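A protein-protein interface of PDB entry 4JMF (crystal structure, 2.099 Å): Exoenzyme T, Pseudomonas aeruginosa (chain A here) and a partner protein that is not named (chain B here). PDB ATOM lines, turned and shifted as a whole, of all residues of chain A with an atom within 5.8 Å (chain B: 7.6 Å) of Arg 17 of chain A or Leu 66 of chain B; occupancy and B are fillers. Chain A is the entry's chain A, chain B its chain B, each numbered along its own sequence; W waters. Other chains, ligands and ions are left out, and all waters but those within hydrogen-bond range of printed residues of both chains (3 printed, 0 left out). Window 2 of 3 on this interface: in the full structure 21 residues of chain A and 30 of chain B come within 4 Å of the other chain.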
ATOM      1  N   GLN A  13      -9.900  -6.301 -20.187  1.00  0.00           N
ATOM      2  CA  GLN A  13      -9.271  -5.363 -19.263  1.00  0.00           C
ATOM      3  C   GLN A  13     -10.305  -4.534 -18.509  1.00  0.00           C
ATOM      4  O   GLN A  13     -10.200  -4.362 -17.285  1.00  0.00           O
ATOM      5  CB  GLN A  13      -8.269  -4.454 -19.989  1.00  0.00           C
ATOM      6  CG  GLN A  13      -6.959  -5.153 -20.373  1.00  0.00           C
ATOM      7  CD  GLN A  13      -6.222  -5.743 -19.166  1.00  0.00           C
ATOM      8  OE1 GLN A  13      -6.455  -6.895 -18.776  1.00  0.00           O
ATOM      9  NE2 GLN A  13      -5.324  -4.952 -18.574  1.00  0.00           N
ATOM     10  N   LEU A  14     -11.301  -4.033 -19.233  1.00  0.00           N
ATOM     11  CA  LEU A  14     -12.361  -3.237 -18.612  1.00  0.00           C
ATOM     12  C   LEU A  14     -13.077  -4.019 -17.511  1.00  0.00           C
ATOM     13  O   LEU A  14     -13.379  -3.482 -16.447  1.00  0.00           O
ATOM     14  CB  LEU A  14     -13.373  -2.765 -19.664  1.00  0.00           C
ATOM     15  CG  LEU A  14     -13.067  -1.429 -20.348  1.00  0.00           C
ATOM     16  CD1 LEU A  14     -14.038  -1.148 -21.487  1.00  0.00           C
ATOM     17  CD2 LEU A  14     -13.089  -0.289 -19.330  1.00  0.00           C
ATOM     18  N   ALA A  15     -13.308  -5.299 -17.776  1.00  0.00           N
ATOM     19  CA  ALA A  15     -14.120  -6.153 -16.928  1.00  0.00           C
ATOM     20  C   ALA A  15     -13.489  -6.434 -15.561  1.00  0.00           C
ATOM     21  O   ALA A  15     -14.141  -6.999 -14.678  1.00  0.00           O
ATOM     22  CB  ALA A  15     -14.412  -7.446 -17.654  1.00  0.00           C
ATOM     23  N   GLN A  16     -12.231  -6.042 -15.386  1.00  0.00           N
ATOM     24  CA  GLN A  16     -11.585  -6.178 -14.083  1.00  0.00           C
ATOM     25  C   GLN A  16     -10.950  -4.869 -13.595  1.00  0.00           C
ATOM     26  O   GLN A  16     -10.062  -4.877 -12.735  1.00  0.00           O
ATOM     27  CB  GLN A  16     -10.565  -7.325 -14.099  1.00  0.00           C
ATOM     28  CG  GLN A  16      -9.443  -7.167 -15.123  1.00  0.00           C
ATOM     29  CD  GLN A  16      -8.754  -8.493 -15.452  1.00  0.00           C
ATOM     30  OE1 GLN A  16      -9.335  -9.574 -15.276  1.00  0.00           O
ATOM     31  NE2 GLN A  16      -7.514  -8.414 -15.940  1.00  0.00           N
ATOM     32  N   ARG A  17     -11.429  -3.743 -14.112  1.00  0.00           N
ATOM     33  CA  ARG A  17     -10.886  -2.452 -13.698  1.00  0.00           C
ATOM     34  C   ARG A  17     -10.980  -2.216 -12.183  1.00  0.00           C
ATOM     35  O   ARG A  17     -12.004  -2.509 -11.549  1.00  0.00           O
ATOM     36  CB  ARG A  17     -11.526  -1.302 -14.487  1.00  0.00           C
ATOM     37  CG  ARG A  17     -12.982  -1.015 -14.177  1.00  0.00           C
ATOM     38  CD  ARG A  17     -13.490   0.103 -15.096  1.00  0.00           C
ATOM     39  NE  ARG A  17     -12.533   1.210 -15.157  1.00  0.00           N
ATOM     40  CZ  ARG A  17     -12.528   2.235 -14.311  1.00  0.00           C
ATOM     41  NH1 ARG A  17     -13.438   2.308 -13.337  1.00  0.00           N
ATOM     42  NH2 ARG A  17     -11.624   3.193 -14.442  1.00  0.00           N
ATOM     43  N   GLN A  18      -9.885  -1.713 -11.617  1.00  0.00           N
ATOM     44  CA  GLN A  18      -9.785  -1.397 -10.193  1.00  0.00           C
ATOM     45  C   GLN A  18      -9.571   0.096 -10.050  1.00  0.00           C
ATOM     46  O   GLN A  18      -8.849   0.692 -10.845  1.00  0.00           O
ATOM     47  CB  GLN A  18      -8.568  -2.097  -9.571  1.00  0.00           C
ATOM     48  CG  GLN A  18      -8.557  -3.605  -9.682  1.00  0.00           C
ATOM     49  CD  GLN A  18      -9.452  -4.252  -8.653  1.00  0.00           C
ATOM     50  OE1 GLN A  18      -9.747  -3.655  -7.613  1.00  0.00           O
ATOM     51  NE2 GLN A  18      -9.901  -5.476  -8.937  1.00  0.00           N
ATOM     52  N   GLU A  19     -10.194   0.706  -9.049  1.00  0.00           N
ATOM     53  CA  GLU A  19      -9.832   2.064  -8.648  1.00  0.00           C
ATOM     54  C   GLU A  19      -9.273   1.963  -7.230  1.00  0.00           C
ATOM     55  O   GLU A  19      -9.632   1.051  -6.485  1.00  0.00           O
ATOM     56  CB  GLU A  19     -11.049   3.000  -8.672  1.00  0.00           C
ATOM     57  CG  GLU A  19     -11.605   3.286 -10.055  1.00  0.00           C
ATOM     58  CD  GLU A  19     -12.913   4.071 -10.034  1.00  0.00           C
ATOM     59  OE1 GLU A  19     -13.237   4.705  -9.007  1.00  0.00           O
ATOM     60  OE2 GLU A  19     -13.628   4.047 -11.055  1.00  0.00           O
ATOM     61  N   THR B  60     -23.202  12.937 -16.770  1.00  0.00           N
ATOM     62  CA  THR B  60     -23.365  12.345 -18.098  1.00  0.00           C
ATOM     63  C   THR B  60     -22.544  11.056 -18.208  1.00  0.00           C
ATOM     64  O   THR B  60     -22.333  10.355 -17.203  1.00  0.00           O
ATOM     65  CB  THR B  60     -23.007  13.369 -19.234  1.00  0.00           C
ATOM     66  OG1 THR B  60     -21.589  13.505 -19.342  1.00  0.00           O
ATOM     67  CG2 THR B  60     -23.582  14.731 -18.914  1.00  0.00           C
ATOM     68  N   ALA B  61     -22.093  10.729 -19.418  1.00  0.00           N
ATOM     69  CA  ALA B  61     -21.203   9.583 -19.603  1.00  0.00           C
ATOM     70  C   ALA B  61     -19.809   9.947 -19.088  1.00  0.00           C
ATOM     71  O   ALA B  61     -18.985  10.510 -19.818  1.00  0.00           O
ATOM     72  CB  ALA B  61     -21.144   9.166 -21.078  1.00  0.00           C
ATOM     73  N   ASN B  62     -19.540   9.637 -17.822  1.00  0.00           N
ATOM     74  CA  ASN B  62     -18.260  10.014 -17.239  1.00  0.00           C
ATOM     75  C   ASN B  62     -17.637   8.948 -16.366  1.00  0.00           C
ATOM     76  O   ASN B  62     -18.198   7.854 -16.187  1.00  0.00           O
ATOM     77  CB  ASN B  62     -18.456  11.236 -16.384  1.00  0.00           C
ATOM     78  CG  ASN B  62     -19.607  11.063 -15.475  1.00  0.00           C
ATOM     79  OD1 ASN B  62     -19.558  10.271 -14.537  1.00  0.00           O
ATOM     80  ND2 ASN B  62     -20.692  11.752 -15.771  1.00  0.00           N
ATOM     81  N   GLU B  63     -16.484   9.308 -15.802  1.00  0.00           N
ATOM     82  CA  GLU B  63     -15.675   8.402 -15.000  1.00  0.00           C
ATOM     83  C   GLU B  63     -16.415   8.036 -13.710  1.00  0.00           C
ATOM     84  O   GLU B  63     -16.375   6.888 -13.269  1.00  0.00           O
ATOM     85  CB  GLU B  63     -14.319   9.044 -14.693  1.00  0.00           C
ATOM     86  CG  GLU B  63     -13.334   8.117 -13.986  1.00  0.00           C
ATOM     87  CD  GLU B  63     -12.025   8.804 -13.627  1.00  0.00           C
ATOM     88  OE1 GLU B  63     -11.831   9.978 -14.016  1.00  0.00           O
ATOM     89  OE2 GLU B  63     -11.193   8.165 -12.946  1.00  0.00           O
ATOM     90  N   GLN B  64     -17.103   9.004 -13.117  1.00  0.00           N
ATOM     91  CA  GLN B  64     -17.865   8.726 -11.906  1.00  0.00           C
ATOM     92  C   GLN B  64     -18.936   7.669 -12.182  1.00  0.00           C
ATOM     93  O   GLN B  64     -19.238   6.834 -11.322  1.00  0.00           O
ATOM     94  CB  GLN B  64     -18.510  10.006 -11.372  1.00  0.00           C
ATOM     95  CG  GLN B  64     -19.211   9.811 -10.025  1.00  0.00           C
ATOM     96  CD  GLN B  64     -18.234   9.425  -8.929  1.00  0.00           C
ATOM     97  OE1 GLN B  64     -17.261  10.134  -8.672  1.00  0.00           O
ATOM     98  NE2 GLN B  64     -18.480   8.281  -8.283  1.00  0.00           N
ATOM     99  N   ASN B  65     -19.483   7.690 -13.395  1.00  0.00           N
ATOM    100  CA  ASN B  65     -20.573   6.781 -13.757  1.00  0.00           C
ATOM    101  C   ASN B  65     -20.136   5.475 -14.428  1.00  0.00           C
ATOM    102  O   ASN B  65     -20.963   4.710 -14.953  1.00  0.00           O
ATOM    103  CB  ASN B  65     -21.629   7.532 -14.575  1.00  0.00           C
ATOM    104  CG  ASN B  65     -22.353   8.573 -13.734  1.00  0.00           C
ATOM    105  OD1 ASN B  65     -22.562   8.365 -12.540  1.00  0.00           O
ATOM    106  ND2 ASN B  65     -22.702   9.706 -14.338  1.00  0.00           N
ATOM    107  N   LEU B  66     -18.833   5.224 -14.397  1.00  0.00           N
ATOM    108  CA  LEU B  66     -18.286   3.938 -14.823  1.00  0.00           C
ATOM    109  C   LEU B  66     -18.133   3.034 -13.603  1.00  0.00           C
ATOM    110  O   LEU B  66     -17.774   3.495 -12.509  1.00  0.00           O
ATOM    111  CB  LEU B  66     -16.914   4.133 -15.470  1.00  0.00           C
ATOM    112  CG  LEU B  66     -16.274   2.889 -16.079  1.00  0.00           C
ATOM    113  CD1 LEU B  66     -17.218   2.311 -17.117  1.00  0.00           C
ATOM    114  CD2 LEU B  66     -14.934   3.241 -16.702  1.00  0.00           C
ATOM    115  N   PHE B  67     -18.417   1.752 -13.782  1.00  0.00           N
ATOM    116  CA  PHE B  67     -18.281   0.789 -12.694  1.00  0.00           C
ATOM    117  C   PHE B  67     -16.819   0.687 -12.242  1.00  0.00           C
ATOM    118  O   PHE B  67     -15.903   0.917 -13.035  1.00  0.00           O
ATOM    119  CB  PHE B  67     -18.799  -0.585 -13.137  1.00  0.00           C
ATOM    120  CG  PHE B  67     -18.093  -1.142 -14.345  1.00  0.00           C
ATOM    121  CD1 PHE B  67     -18.652  -1.015 -15.618  1.00  0.00           C
ATOM    122  CD2 PHE B  67     -16.876  -1.799 -14.212  1.00  0.00           C
ATOM    123  CE1 PHE B  67     -18.002  -1.536 -16.740  1.00  0.00           C
ATOM    124  CE2 PHE B  67     -16.214  -2.316 -15.330  1.00  0.00           C
ATOM    125  CZ  PHE B  67     -16.783  -2.187 -16.591  1.00  0.00           C
ATOM    126  N   SER B  68     -16.606   0.360 -10.969  1.00  0.00           N
ATOM    127  CA  SER B  68     -15.287  -0.054 -10.499  1.00  0.00           C
ATOM    128  C   SER B  68     -15.460  -1.404  -9.834  1.00  0.00           C
ATOM    129  O   SER B  68     -16.489  -2.047 -10.017  1.00  0.00           O
ATOM    130  CB  SER B  68     -14.697   0.950  -9.511  1.00  0.00           C
ATOM    131  OG  SER B  68     -15.273   0.792  -8.229  1.00  0.00           O
ATOM    132  N   GLN B  69     -14.475  -1.829  -9.047  1.00  0.00           N
ATOM    133  CA  GLN B  69     -14.595  -3.098  -8.325  1.00  0.00           C
ATOM    134  C   GLN B  69     -15.518  -2.987  -7.110  1.00  0.00           C
ATOM    135  O   GLN B  69     -15.920  -4.009  -6.542  1.00  0.00           O
ATOM    136  CB  GLN B  69     -13.218  -3.619  -7.892  1.00  0.00           C
ATOM    137  CG  GLN B  69     -12.679  -2.997  -6.609  1.00  0.00           C
ATOM    138  CD  GLN B  69     -12.253  -1.544  -6.773  1.00  0.00           C
ATOM    139  OE1 GLN B  69     -12.153  -1.024  -7.887  1.00  0.00           O
ATOM    140  NE2 GLN B  69     -12.019  -0.871  -5.648  1.00  0.00           N
ATOM    141  N   ASP B  70     -15.867  -1.760  -6.723  1.00  0.00           N
ATOM    142  CA  ASP B  70     -16.696  -1.542  -5.527  1.00  0.00           C
ATOM    143  C   ASP B  70     -18.113  -1.157  -5.922  1.00  0.00           C
ATOM    144  O   ASP B  70     -18.337  -0.048  -6.409  1.00  0.00           O
ATOM    145  CB  ASP B  70     -16.093  -0.417  -4.668  1.00  0.00           C
ATOM    146  CG  ASP B  70     -16.738  -0.312  -3.293  1.00  0.00           C
ATOM    147  OD1 ASP B  70     -17.904  -0.748  -3.127  1.00  0.00           O
ATOM    148  OD2 ASP B  70     -16.073   0.212  -2.368  1.00  0.00           O
ATOM    149  N   LYS B  73     -19.678   2.310  -5.173  1.00  0.00           N
ATOM    150  CA  LYS B  73     -19.224   3.549  -5.832  1.00  0.00           C
ATOM    151  C   LYS B  73     -20.484   4.226  -6.339  1.00  0.00           C
ATOM    152  O   LYS B  73     -21.296   3.592  -7.022  1.00  0.00           O
ATOM    153  CB  LYS B  73     -18.293   3.260  -7.005  1.00  0.00           C
ATOM    154  CG  LYS B  73     -17.902   4.524  -7.778  1.00  0.00           C
ATOM    155  CD  LYS B  73     -17.146   4.184  -9.046  1.00  0.00           C
ATOM    156  CE  LYS B  73     -16.735   5.468  -9.780  1.00  0.00           C
ATOM    157  NZ  LYS B  73     -15.950   5.183 -11.015  1.00  0.00           N
ATOM    158  N   PRO B  74     -20.690   5.493  -5.961  1.00  0.00           N
ATOM    159  CA  PRO B  74     -21.981   6.102  -6.294  1.00  0.00           C
ATOM    160  C   PRO B  74     -22.074   6.561  -7.745  1.00  0.00           C
ATOM    161  O   PRO B  74     -21.072   6.657  -8.463  1.00  0.00           O
ATOM    162  CB  PRO B  74     -22.058   7.309  -5.348  1.00  0.00           C
ATOM    163  CG  PRO B  74     -20.631   7.645  -5.068  1.00  0.00           C
ATOM    164  CD  PRO B  74     -19.838   6.381  -5.154  1.00  0.00           C
ATOM    165  N   ILE B  75     -23.304   6.847  -8.155  1.00  0.00           N
ATOM    166  CA  ILE B  75     -23.623   7.208  -9.519  1.00  0.00           C
ATOM    167  C   ILE B  75     -24.144   8.641  -9.467  1.00  0.00           C
ATOM    168  O   ILE B  75     -24.783   9.019  -8.488  1.00  0.00           O
ATOM    169  CB  ILE B  75     -24.748   6.291 -10.032  1.00  0.00           C
ATOM    170  CG1 ILE B  75     -24.351   4.829  -9.873  1.00  0.00           C
ATOM    171  CG2 ILE B  75     -25.136   6.613 -11.474  1.00  0.00           C
ATOM    172  CD1 ILE B  75     -23.066   4.504 -10.520  1.00  0.00           C
HETATM  173  O   HOH W   1     -11.542   5.359 -13.061  1.00  0.00           O
HETATM  174  O   HOH W   2     -12.424   2.079  -4.994  1.00  0.00           O
HETATM  175  O   HOH W   3     -14.545   2.739  -6.514  1.00  0.00           O
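Among the printed residues, merely in contact across the chains: Leu 14 of chain A with Phe 67 of chain B, Arg 17 of chain A with Leu 66 of chain B, Arg 17 of chain A with Gln 69 of chain B, Gln 18 of chain A with Gln 69 of chain B and Glu 19 of chain A with Ser 68 of chain B.
N of Glu 19 of chain A lies within hydrogen-bond range of OE1 of Gln 69 of chain B, 2.9 Å away.
The side-chain carboxylate (OE2) of Glu 19 of chain A lies within salt-bridge range of the side-chain amino group (NZ) of Lys 73 of chain B, 2.6 Å away.
NH1 of Arg 17 of chain A lies within hydrogen-bond range of O of Phe 67 of chain B (2.8 Å).
Water W1 lies within hydrogen-bond range of NH2 of Arg 17 of chain A (2.6 Å), OE2 of Glu 63 of chain B (2.8 Å) and OE2 of Glu 19 of chain A (3.2 Å).
Water W3 bridges OG of Ser 68 of chain B (2.7 Å) and OE1 of Glu 19 of chain A (3.4 Å).
Water W2 bridges NE2 of Gln 69 of chain B (3.0 Å) and O of Glu 19 of chain A (3.3 Å).
Of the printed residues of chain B, Arg 17 of chain A touches Leu 66 (3.5 Å), Phe 67 (2.8 Å) and Gln 69 (3.6 Å).
Of the printed residues of chain B, Gln 18 of chain A touches Gln 69.
Of the printed residues of chain B, Glu 19 of chain A touches Ser 68, Gln 69 and Lys 73.
Leu 66 of chain B touches one residue of chain A.
Of the printed residues of chain A, Ser 68 of chain B touches Glu 19 (3.6 Å).
Of the printed residues of chain A, Gln 69 of chain B touches Arg 17, Gln 18 and Glu 19.
Printed residues of chain A within 4 Å of Lys 73 of chain B: Glu 19 (2.6 Å).
The nearest printed residue of chain B that does not touch Arg 17 of chain A is Ser 68 of chain B (4.01 Å).
The nearest residue of chain A that does not touch Leu 66 of chain B is Glu 19 of chain A (4.4 Å).
The side-chain hydroxyl (OG) of Ser 68 of chain B is in hydrogen-bond range of the backbone NH (N) of Asp 70 of chain B (3.0 Å).
O of Glu 63 of chain B lies within hydrogen-bond range of NZ of Lys 73 of chain B.
The guanidinium group (NH1) of Arg 17 of chain A lies within salt-bridge range of the side-chain carboxylate (OE2) of Glu 19 of chain A (2.9 Å).
NZ of Lys 73 of chain B sits at hydrogen-bond distance from O of Leu 66 of chain B, at 2.9 Å.
Printed residues of chain B that touch a printed residue of chain A: Leu 66, Phe 67, Ser 68, Gln 69 and Lys 73.
Hydrophobic or aromatic side chains of chain B that line the printed part of chain A: Leu 66 and Phe 67.
Among the printed residues, 8 pairs touch across the chains.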
